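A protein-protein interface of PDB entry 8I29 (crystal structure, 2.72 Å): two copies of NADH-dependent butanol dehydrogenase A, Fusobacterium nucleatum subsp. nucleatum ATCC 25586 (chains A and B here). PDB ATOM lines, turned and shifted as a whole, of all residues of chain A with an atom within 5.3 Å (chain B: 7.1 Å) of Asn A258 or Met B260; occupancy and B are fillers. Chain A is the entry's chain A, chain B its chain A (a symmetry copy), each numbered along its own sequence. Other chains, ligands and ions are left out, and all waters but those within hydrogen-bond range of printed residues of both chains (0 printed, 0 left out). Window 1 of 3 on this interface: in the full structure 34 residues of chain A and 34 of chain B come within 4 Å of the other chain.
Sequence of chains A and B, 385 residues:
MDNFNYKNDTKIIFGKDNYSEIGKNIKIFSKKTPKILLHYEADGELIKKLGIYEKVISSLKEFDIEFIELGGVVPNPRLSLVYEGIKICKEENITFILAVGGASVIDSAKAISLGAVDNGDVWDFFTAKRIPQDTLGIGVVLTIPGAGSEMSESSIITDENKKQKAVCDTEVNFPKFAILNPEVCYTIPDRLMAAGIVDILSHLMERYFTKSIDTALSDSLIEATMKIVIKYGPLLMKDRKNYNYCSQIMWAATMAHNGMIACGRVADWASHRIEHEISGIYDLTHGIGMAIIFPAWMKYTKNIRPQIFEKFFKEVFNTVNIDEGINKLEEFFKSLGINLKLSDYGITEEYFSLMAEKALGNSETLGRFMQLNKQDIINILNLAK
The backbone carbonyl oxygen (O) of Met B260 sits at hydrogen-bond distance from the side-chain sulfur (SG) of Cys B263.
OH of Tyr A6 sits at hydrogen-bond distance from ND2 of Asn A258, 3.0 Å away.
The side-chain amide oxygen (OD1) of Asn A258 lies close to the backbone NH (N) of Met A260 (3.2 Å).
ND2 of Asn B258 lies within hydrogen-bond range of OH of Tyr B6, 3.0 Å away.
The backbone NH (N) of Met B260 sits close to the side-chain amide oxygen (OD1) of Asn B258, at 3.2 Å.
Hydrophobic or aromatic side chains of chain B within 4 Å of the printed part of chain A: Phe B4, Leu B217, Leu B221, Met B255 and Met B260.
Along chain B the printed residues that touch a printed residue of chain A span positions 4 to 263.
Hydrophobic or aromatic side chains of chain A that line the printed part of chain B: Ile A12, Trp A251, Met A255 and Met A260.
Along chain A the printed residues that touch a printed residue of chain B span positions 12 to 260.
Among the printed residues, no Asp or Glu carboxylate lies within 4 Å of a Lys or Arg side-chain nitrogen of the other chain.
Among the printed residues, pairs that only touch across the chains: Ile A12 with Phe B4 (3.98 Å), Trp A251 with Phe B4 (3.5 Å), Trp A251 with Leu B217 (3.4 Å) and Met A255 with Leu B221 (3.7 Å).
ND2 of Asn B258 sits at hydrogen-bond distance from SD of Met A260 (3.5 Å).
The backbone NH of Ile A12 is in hydrogen-bond range of the backbone carbonyl oxygen of Tyr B6 (2.8 Å).
The side-chain amide nitrogen of Asn A258 sits at hydrogen-bond distance from the side-chain sulfur of Met B260, at 3.5 Å.
NE1 of Trp A251 lies within hydrogen-bond range of O of Met B260, at 3.1 Å.
SG of Cys B263 is in hydrogen-bond range of NE1 of Trp A251 (2.8 Å).
The side-chain sulfur of Met A255 sits close to the backbone carbonyl oxygen of Met B260 (3.7 Å).
The side-chain sulfur (SD) of Met B255 sits close to the backbone carbonyl oxygen (O) of Met A260 (3.7 Å).
Of the printed residues of chain B, Ile A12 touches Phe B4 (3.98 Å) and Tyr B6 (2.8 Å).
Of the printed residues of chain B, Asn A258 touches Met B260.
Of the printed residues of chain A, Tyr B6 touches Ile A12 (2.8 Å).
Of the printed residues of chain A, Leu B221 touches Met A255.
Met B260 touches just these residues of chain A: Trp A251, Met A255 and Asn A258.
The nearest residue of chain B that does not touch Asn A258 is Asn B258 (5.3 Å).
The nearest printed residue of chain A that does not touch Met B255 is Ile A261 (4.1 Å).
Met A255 touches Met B260, and with the chains exchanged Met A260 touches Met B255.
Asn A258 touches Met B260, and with the chains exchanged Met A260 touches Asn B258.
Positions printed for both chains: 6, 255, 257, 258, 259, 260, 261 and 262.
Of the 11 pairs that touch across the chains among the printed residues, 4 have their exchanged pair printed and touching as well.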
ATOM      1  N   TYR A   6       5.592  39.631  -8.504  1.00  0.00           N
ATOM      2  CA  TYR A   6       6.443  38.467  -8.641  1.00  0.00           C
ATOM      3  C   TYR A   6       7.665  38.765  -9.508  1.00  0.00           C
ATOM      4  O   TYR A   6       7.523  39.130 -10.679  1.00  0.00           O
ATOM      5  CB  TYR A   6       5.676  37.293  -9.245  1.00  0.00           C
ATOM      6  CG  TYR A   6       6.556  36.102  -9.549  1.00  0.00           C
ATOM      7  CD1 TYR A   6       6.972  35.225  -8.547  1.00  0.00           C
ATOM      8  CD2 TYR A   6       7.021  35.883 -10.840  1.00  0.00           C
ATOM      9  CE1 TYR A   6       7.796  34.143  -8.830  1.00  0.00           C
ATOM     10  CE2 TYR A   6       7.838  34.803 -11.141  1.00  0.00           C
ATOM     11  CZ  TYR A   6       8.225  33.929 -10.134  1.00  0.00           C
ATOM     12  OH  TYR A   6       9.046  32.868 -10.462  1.00  0.00           O
ATOM     13  N   ILE A  12      17.493  28.253 -13.642  1.00  0.00           N
ATOM     14  CA  ILE A  12      17.371  26.895 -13.158  1.00  0.00           C
ATOM     15  C   ILE A  12      17.851  25.981 -14.272  1.00  0.00           C
ATOM     16  O   ILE A  12      17.322  26.052 -15.385  1.00  0.00           O
ATOM     17  CB  ILE A  12      15.928  26.592 -12.720  1.00  0.00           C
ATOM     18  CG1 ILE A  12      15.603  27.240 -11.375  1.00  0.00           C
ATOM     19  CG2 ILE A  12      15.669  25.096 -12.670  1.00  0.00           C
ATOM     20  CD1 ILE A  12      14.132  27.164 -11.008  1.00  0.00           C
ATOM     21  N   MET A 151      16.789  29.412  -4.535  1.00  0.00           N
ATOM     22  CA  MET A 151      15.903  30.177  -5.384  1.00  0.00           C
ATOM     23  C   MET A 151      15.240  31.304  -4.593  1.00  0.00           C
ATOM     24  O   MET A 151      14.336  31.943  -5.115  1.00  0.00           O
ATOM     25  CB  MET A 151      14.842  29.215  -5.894  1.00  0.00           C
ATOM     26  CG  MET A 151      14.503  29.355  -7.344  1.00  0.00           C
ATOM     27  SD  MET A 151      12.888  28.592  -7.621  1.00  0.00           S
ATOM     28  CE  MET A 151      12.919  27.281  -6.391  1.00  0.00           C
ATOM     29  N   TRP A 251      10.849  18.607  -8.680  1.00  0.00           N
ATOM     30  CA  TRP A 251      10.243  19.685  -9.436  1.00  0.00           C
ATOM     31  C   TRP A 251       9.070  20.234  -8.634  1.00  0.00           C
ATOM     32  O   TRP A 251       8.802  21.425  -8.726  1.00  0.00           O
ATOM     33  CB  TRP A 251       9.863  19.285 -10.871  1.00  0.00           C
ATOM     34  CG  TRP A 251       9.537  20.482 -11.715  1.00  0.00           C
ATOM     35  CD1 TRP A 251       8.377  20.724 -12.393  1.00  0.00           C
ATOM     36  CD2 TRP A 251      10.366  21.638 -11.941  1.00  0.00           C
ATOM     37  NE1 TRP A 251       8.434  21.937 -13.030  1.00  0.00           N
ATOM     38  CE2 TRP A 251       9.633  22.526 -12.758  1.00  0.00           C
ATOM     39  CE3 TRP A 251      11.662  21.992 -11.568  1.00  0.00           C
ATOM     40  CZ2 TRP A 251      10.136  23.751 -13.179  1.00  0.00           C
ATOM     41  CZ3 TRP A 251      12.151  23.217 -11.962  1.00  0.00           C
ATOM     42  CH2 TRP A 251      11.403  24.088 -12.754  1.00  0.00           C
ATOM     43  N   THR A 254      10.632  22.679  -5.904  1.00  0.00           N
ATOM     44  CA  THR A 254      10.910  23.906  -6.637  1.00  0.00           C
ATOM     45  C   THR A 254       9.624  24.724  -6.844  1.00  0.00           C
ATOM     46  O   THR A 254       9.544  25.871  -6.388  1.00  0.00           O
ATOM     47  CB  THR A 254      11.604  23.586  -7.966  1.00  0.00           C
ATOM     48  OG1 THR A 254      12.804  22.877  -7.644  1.00  0.00           O
ATOM     49  CG2 THR A 254      11.881  24.819  -8.801  1.00  0.00           C
ATOM     50  N   MET A 255       8.615  24.110  -7.499  1.00  0.00           N
ATOM     51  CA  MET A 255       7.343  24.766  -7.780  1.00  0.00           C
ATOM     52  C   MET A 255       6.684  25.231  -6.478  1.00  0.00           C
ATOM     53  O   MET A 255       6.150  26.340  -6.438  1.00  0.00           O
ATOM     54  CB  MET A 255       6.356  23.882  -8.555  1.00  0.00           C
ATOM     55  CG  MET A 255       6.758  23.587 -10.007  1.00  0.00           C
ATOM     56  SD  MET A 255       6.659  24.996 -11.104  1.00  0.00           S
ATOM     57  CE  MET A 255       4.907  25.347 -11.098  1.00  0.00           C
ATOM     58  N   ALA A 256       6.749  24.424  -5.408  1.00  0.00           N
ATOM     59  CA  ALA A 256       6.215  24.863  -4.129  1.00  0.00           C
ATOM     60  C   ALA A 256       6.857  26.179  -3.678  1.00  0.00           C
ATOM     61  O   ALA A 256       6.189  27.004  -3.087  1.00  0.00           O
ATOM     62  CB  ALA A 256       6.366  23.779  -3.097  1.00  0.00           C
ATOM     63  N   HIS A 257       8.132  26.419  -3.991  1.00  0.00           N
ATOM     64  CA  HIS A 257       8.774  27.691  -3.662  1.00  0.00           C
ATOM     65  C   HIS A 257       8.510  28.776  -4.708  1.00  0.00           C
ATOM     66  O   HIS A 257       9.171  29.803  -4.747  1.00  0.00           O
ATOM     67  CB  HIS A 257      10.268  27.465  -3.436  1.00  0.00           C
ATOM     68  CG  HIS A 257      10.444  26.539  -2.310  1.00  0.00           C
ATOM     69  ND1 HIS A 257      11.104  25.337  -2.416  1.00  0.00           N
ATOM     70  CD2 HIS A 257       9.992  26.641  -1.060  1.00  0.00           C
ATOM     71  CE1 HIS A 257      11.047  24.730  -1.244  1.00  0.00           C
ATOM     72  NE2 HIS A 257      10.373  25.507  -0.408  1.00  0.00           N
ATOM     73  N   ASN A 258       7.487  28.584  -5.521  1.00  0.00           N
ATOM     74  CA  ASN A 258       7.157  29.544  -6.551  1.00  0.00           C
ATOM     75  C   ASN A 258       5.902  30.303  -6.109  1.00  0.00           C
ATOM     76  O   ASN A 258       4.964  29.737  -5.533  1.00  0.00           O
ATOM     77  CB  ASN A 258       6.998  28.827  -7.896  1.00  0.00           C
ATOM     78  CG  ASN A 258       7.237  29.733  -9.077  1.00  0.00           C
ATOM     79  OD1 ASN A 258       6.312  30.012  -9.839  1.00  0.00           O
ATOM     80  ND2 ASN A 258       8.464  30.207  -9.214  1.00  0.00           N
ATOM     81  N   GLY A 259       5.911  31.612  -6.367  1.00  0.00           N
ATOM     82  CA  GLY A 259       4.796  32.475  -6.041  1.00  0.00           C
ATOM     83  C   GLY A 259       4.038  32.834  -7.310  1.00  0.00           C
ATOM     84  O   GLY A 259       3.257  33.802  -7.357  1.00  0.00           O
ATOM     85  N   MET A 260       4.274  32.028  -8.347  1.00  0.00           N
ATOM     86  CA  MET A 260       3.371  32.077  -9.473  1.00  0.00           C
ATOM     87  C   MET A 260       2.165  31.185  -9.202  1.00  0.00           C
ATOM     88  O   MET A 260       1.089  31.421  -9.747  1.00  0.00           O
ATOM     89  CB  MET A 260       4.083  31.665 -10.753  1.00  0.00           C
ATOM     90  CG  MET A 260       5.091  32.682 -11.151  1.00  0.00           C
ATOM     91  SD  MET A 260       5.369  32.541 -12.891  1.00  0.00           S
ATOM     92  CE  MET A 260       4.265  33.811 -13.489  1.00  0.00           C
ATOM     93  N   ILE A 261       2.336  30.159  -8.369  1.00  0.00           N
ATOM     94  CA  ILE A 261       1.202  29.309  -8.096  1.00  0.00           C
ATOM     95  C   ILE A 261       0.478  29.859  -6.883  1.00  0.00           C
ATOM     96  O   ILE A 261      -0.734  29.945  -6.935  1.00  0.00           O
ATOM     97  CB  ILE A 261       1.559  27.814  -8.028  1.00  0.00           C
ATOM     98  CG1 ILE A 261       2.592  27.492  -6.947  1.00  0.00           C
ATOM     99  CG2 ILE A 261       1.993  27.323  -9.407  1.00  0.00           C
ATOM    100  CD1 ILE A 261       2.409  26.121  -6.312  1.00  0.00           C
ATOM    101  N   ALA A 262       1.184  30.341  -5.859  1.00  0.00           N
ATOM    102  CA  ALA A 262       0.535  31.102  -4.797  1.00  0.00           C
ATOM    103  C   ALA A 262       0.614  32.570  -5.180  1.00  0.00           C
ATOM    104  O   ALA A 262       1.720  33.085  -5.278  1.00  0.00           O
ATOM    105  CB  ALA A 262       1.210  30.831  -3.480  1.00  0.00           C
ATOM    106  N   PHE B   4      16.081  20.528 -18.890  1.00  0.00           N
ATOM    107  CA  PHE B   4      15.587  21.819 -19.339  1.00  0.00           C
ATOM    108  C   PHE B   4      16.189  22.918 -18.479  1.00  0.00           C
ATOM    109  O   PHE B   4      16.635  22.659 -17.352  1.00  0.00           O
ATOM    110  CB  PHE B   4      14.052  21.887 -19.303  1.00  0.00           C
ATOM    111  CG  PHE B   4      13.459  21.913 -17.922  1.00  0.00           C
ATOM    112  CD1 PHE B   4      13.198  20.733 -17.242  1.00  0.00           C
ATOM    113  CD2 PHE B   4      13.233  23.108 -17.272  1.00  0.00           C
ATOM    114  CE1 PHE B   4      12.693  20.745 -15.952  1.00  0.00           C
ATOM    115  CE2 PHE B   4      12.712  23.121 -15.984  1.00  0.00           C
ATOM    116  CZ  PHE B   4      12.447  21.940 -15.323  1.00  0.00           C
ATOM    117  N   TYR B   6      15.487  27.194 -17.269  1.00  0.00           N
ATOM    118  CA  TYR B   6      14.473  28.218 -17.116  1.00  0.00           C
ATOM    119  C   TYR B   6      15.032  29.461 -16.426  1.00  0.00           C
ATOM    120  O   TYR B   6      15.504  29.381 -15.288  1.00  0.00           O
ATOM    121  CB  TYR B   6      13.281  27.696 -16.318  1.00  0.00           C
ATOM    122  CG  TYR B   6      12.264  28.768 -16.000  1.00  0.00           C
ATOM    123  CD1 TYR B   6      11.344  29.210 -16.953  1.00  0.00           C
ATOM    124  CD2 TYR B   6      12.258  29.384 -14.754  1.00  0.00           C
ATOM    125  CE1 TYR B   6      10.424  30.208 -16.660  1.00  0.00           C
ATOM    126  CE2 TYR B   6      11.341  30.377 -14.445  1.00  0.00           C
ATOM    127  CZ  TYR B   6      10.420  30.790 -15.398  1.00  0.00           C
ATOM    128  OH  TYR B   6       9.525  31.787 -15.062  1.00  0.00           O
ATOM    129  N   LEU B 217       4.010  15.889 -13.173  1.00  0.00           N
ATOM    130  CA  LEU B 217       3.732  17.175 -12.557  1.00  0.00           C
ATOM    131  C   LEU B 217       3.432  18.239 -13.614  1.00  0.00           C
ATOM    132  O   LEU B 217       2.440  18.984 -13.513  1.00  0.00           O
ATOM    133  CB  LEU B 217       4.929  17.577 -11.697  1.00  0.00           C
ATOM    134  CG  LEU B 217       4.916  19.013 -11.199  1.00  0.00           C
ATOM    135  CD1 LEU B 217       3.625  19.289 -10.471  1.00  0.00           C
ATOM    136  CD2 LEU B 217       6.102  19.249 -10.290  1.00  0.00           C
ATOM    137  N   SER B 218       4.300  18.306 -14.627  1.00  0.00           N
ATOM    138  CA  SER B 218       4.070  19.205 -15.743  1.00  0.00           C
ATOM    139  C   SER B 218       2.671  18.986 -16.336  1.00  0.00           C
ATOM    140  O   SER B 218       1.904  19.930 -16.575  1.00  0.00           O
ATOM    141  CB  SER B 218       5.146  19.018 -16.749  1.00  0.00           C
ATOM    142  OG  SER B 218       4.939  19.855 -17.866  1.00  0.00           O
ATOM    143  N   LEU B 221      -0.012  20.562 -14.071  1.00  0.00           N
ATOM    144  CA  LEU B 221      -0.049  22.007 -14.054  1.00  0.00           C
ATOM    145  C   LEU B 221      -0.740  22.485 -15.319  1.00  0.00           C
ATOM    146  O   LEU B 221      -1.642  23.296 -15.200  1.00  0.00           O
ATOM    147  CB  LEU B 221       1.368  22.550 -13.891  1.00  0.00           C
ATOM    148  CG  LEU B 221       2.021  22.205 -12.538  1.00  0.00           C
ATOM    149  CD1 LEU B 221       3.541  22.269 -12.578  1.00  0.00           C
ATOM    150  CD2 LEU B 221       1.525  23.103 -11.417  1.00  0.00           C
ATOM    151  N   MET B 255       0.513  32.371 -17.089  1.00  0.00           N
ATOM    152  CA  MET B 255       1.016  31.049 -16.731  1.00  0.00           C
ATOM    153  C   MET B 255       1.237  30.204 -17.989  1.00  0.00           C
ATOM    154  O   MET B 255       2.251  29.510 -18.077  1.00  0.00           O
ATOM    155  CB  MET B 255       0.098  30.284 -15.767  1.00  0.00           C
ATOM    156  CG  MET B 255       0.027  30.866 -14.348  1.00  0.00           C
ATOM    157  SD  MET B 255       1.524  30.667 -13.389  1.00  0.00           S
ATOM    158  CE  MET B 255       1.628  28.889 -13.232  1.00  0.00           C
ATOM    159  N   HIS B 257       2.323  31.211 -20.728  1.00  0.00           N
ATOM    160  CA  HIS B 257       3.625  31.622 -21.250  1.00  0.00           C
ATOM    161  C   HIS B 257       4.776  31.303 -20.292  1.00  0.00           C
ATOM    162  O   HIS B 257       5.881  31.805 -20.428  1.00  0.00           O
ATOM    163  CB  HIS B 257       3.582  33.103 -21.620  1.00  0.00           C
ATOM    164  CG  HIS B 257       2.568  33.303 -22.662  1.00  0.00           C
ATOM    165  ND1 HIS B 257       1.487  34.141 -22.515  1.00  0.00           N
ATOM    166  CD2 HIS B 257       2.466  32.722 -23.858  1.00  0.00           C
ATOM    167  CE1 HIS B 257       0.751  34.061 -23.608  1.00  0.00           C
ATOM    168  NE2 HIS B 257       1.328  33.201 -24.435  1.00  0.00           N
ATOM    169  N   ASN B 258       4.538  30.405 -19.353  1.00  0.00           N
ATOM    170  CA  ASN B 258       5.554  30.038 -18.392  1.00  0.00           C
ATOM    171  C   ASN B 258       6.080  28.647 -18.761  1.00  0.00           C
ATOM    172  O   ASN B 258       5.329  27.752 -19.170  1.00  0.00           O
ATOM    173  CB  ASN B 258       4.978  30.119 -16.974  1.00  0.00           C
ATOM    174  CG  ASN B 258       6.036  30.335 -15.921  1.00  0.00           C
ATOM    175  OD1 ASN B 258       6.270  29.458 -15.091  1.00  0.00           O
ATOM    176  ND2 ASN B 258       6.686  31.486 -15.971  1.00  0.00           N
ATOM    177  N   GLY B 259       7.397  28.488 -18.635  1.00  0.00           N
ATOM    178  CA  GLY B 259       8.057  27.231 -18.916  1.00  0.00           C
ATOM    179  C   GLY B 259       8.450  26.556 -17.610  1.00  0.00           C
ATOM    180  O   GLY B 259       9.301  25.647 -17.571  1.00  0.00           O
ATOM    181  N   MET B 260       7.807  27.009 -16.533  1.00  0.00           N
ATOM    182  CA  MET B 260       7.858  26.222 -15.322  1.00  0.00           C
ATOM    183  C   MET B 260       6.784  25.141 -15.367  1.00  0.00           C
ATOM    184  O   MET B 260       6.931  24.101 -14.730  1.00  0.00           O
ATOM    185  CB  MET B 260       7.695  27.109 -14.098  1.00  0.00           C
ATOM    186  CG  MET B 260       8.879  27.989 -13.917  1.00  0.00           C
ATOM    187  SD  MET B 260       8.974  28.454 -12.214  1.00  0.00           S
ATOM    188  CE  MET B 260      10.140  27.238 -11.622  1.00  0.00           C
ATOM    189  N   ILE B 261       5.704  25.379 -16.110  1.00  0.00           N
ATOM    190  CA  ILE B 261       4.682  24.363 -16.169  1.00  0.00           C
ATOM    191  C   ILE B 261       4.987  23.450 -17.340  1.00  0.00           C
ATOM    192  O   ILE B 261       4.912  22.251 -17.160  1.00  0.00           O
ATOM    193  CB  ILE B 261       3.251  24.929 -16.130  1.00  0.00           C
ATOM    194  CG1 ILE B 261       2.954  25.888 -17.285  1.00  0.00           C
ATOM    195  CG2 ILE B 261       2.983  25.564 -14.768  1.00  0.00           C
ATOM    196  CD1 ILE B 261       1.508  25.849 -17.758  1.00  0.00           C
ATOM    197  N   ALA B 262       5.442  23.974 -18.480  1.00  0.00           N
ATOM    198  CA  ALA B 262       5.982  23.119 -19.531  1.00  0.00           C
ATOM    199  C   ALA B 262       7.481  23.017 -19.305  1.00  0.00           C
ATOM    200  O   ALA B 262       8.151  24.038 -19.383  1.00  0.00           O
ATOM    201  CB  ALA B 262       5.660  23.695 -20.883  1.00  0.00           C
ATOM    202  N   CYS B 263       8.005  21.827 -18.977  1.00  0.00           N
ATOM    203  CA  CYS B 263       9.389  21.705 -18.522  1.00  0.00           C
ATOM    204  C   CYS B 263      10.253  21.017 -19.589  1.00  0.00           C
ATOM    205  O   CYS B 263      10.635  19.857 -19.420  1.00  0.00           O
ATOM    206  CB  CYS B 263       9.511  20.845 -17.261  1.00  0.00           C
ATOM    207  SG  CYS B 263       8.563  21.346 -15.789  1.00  0.00           S
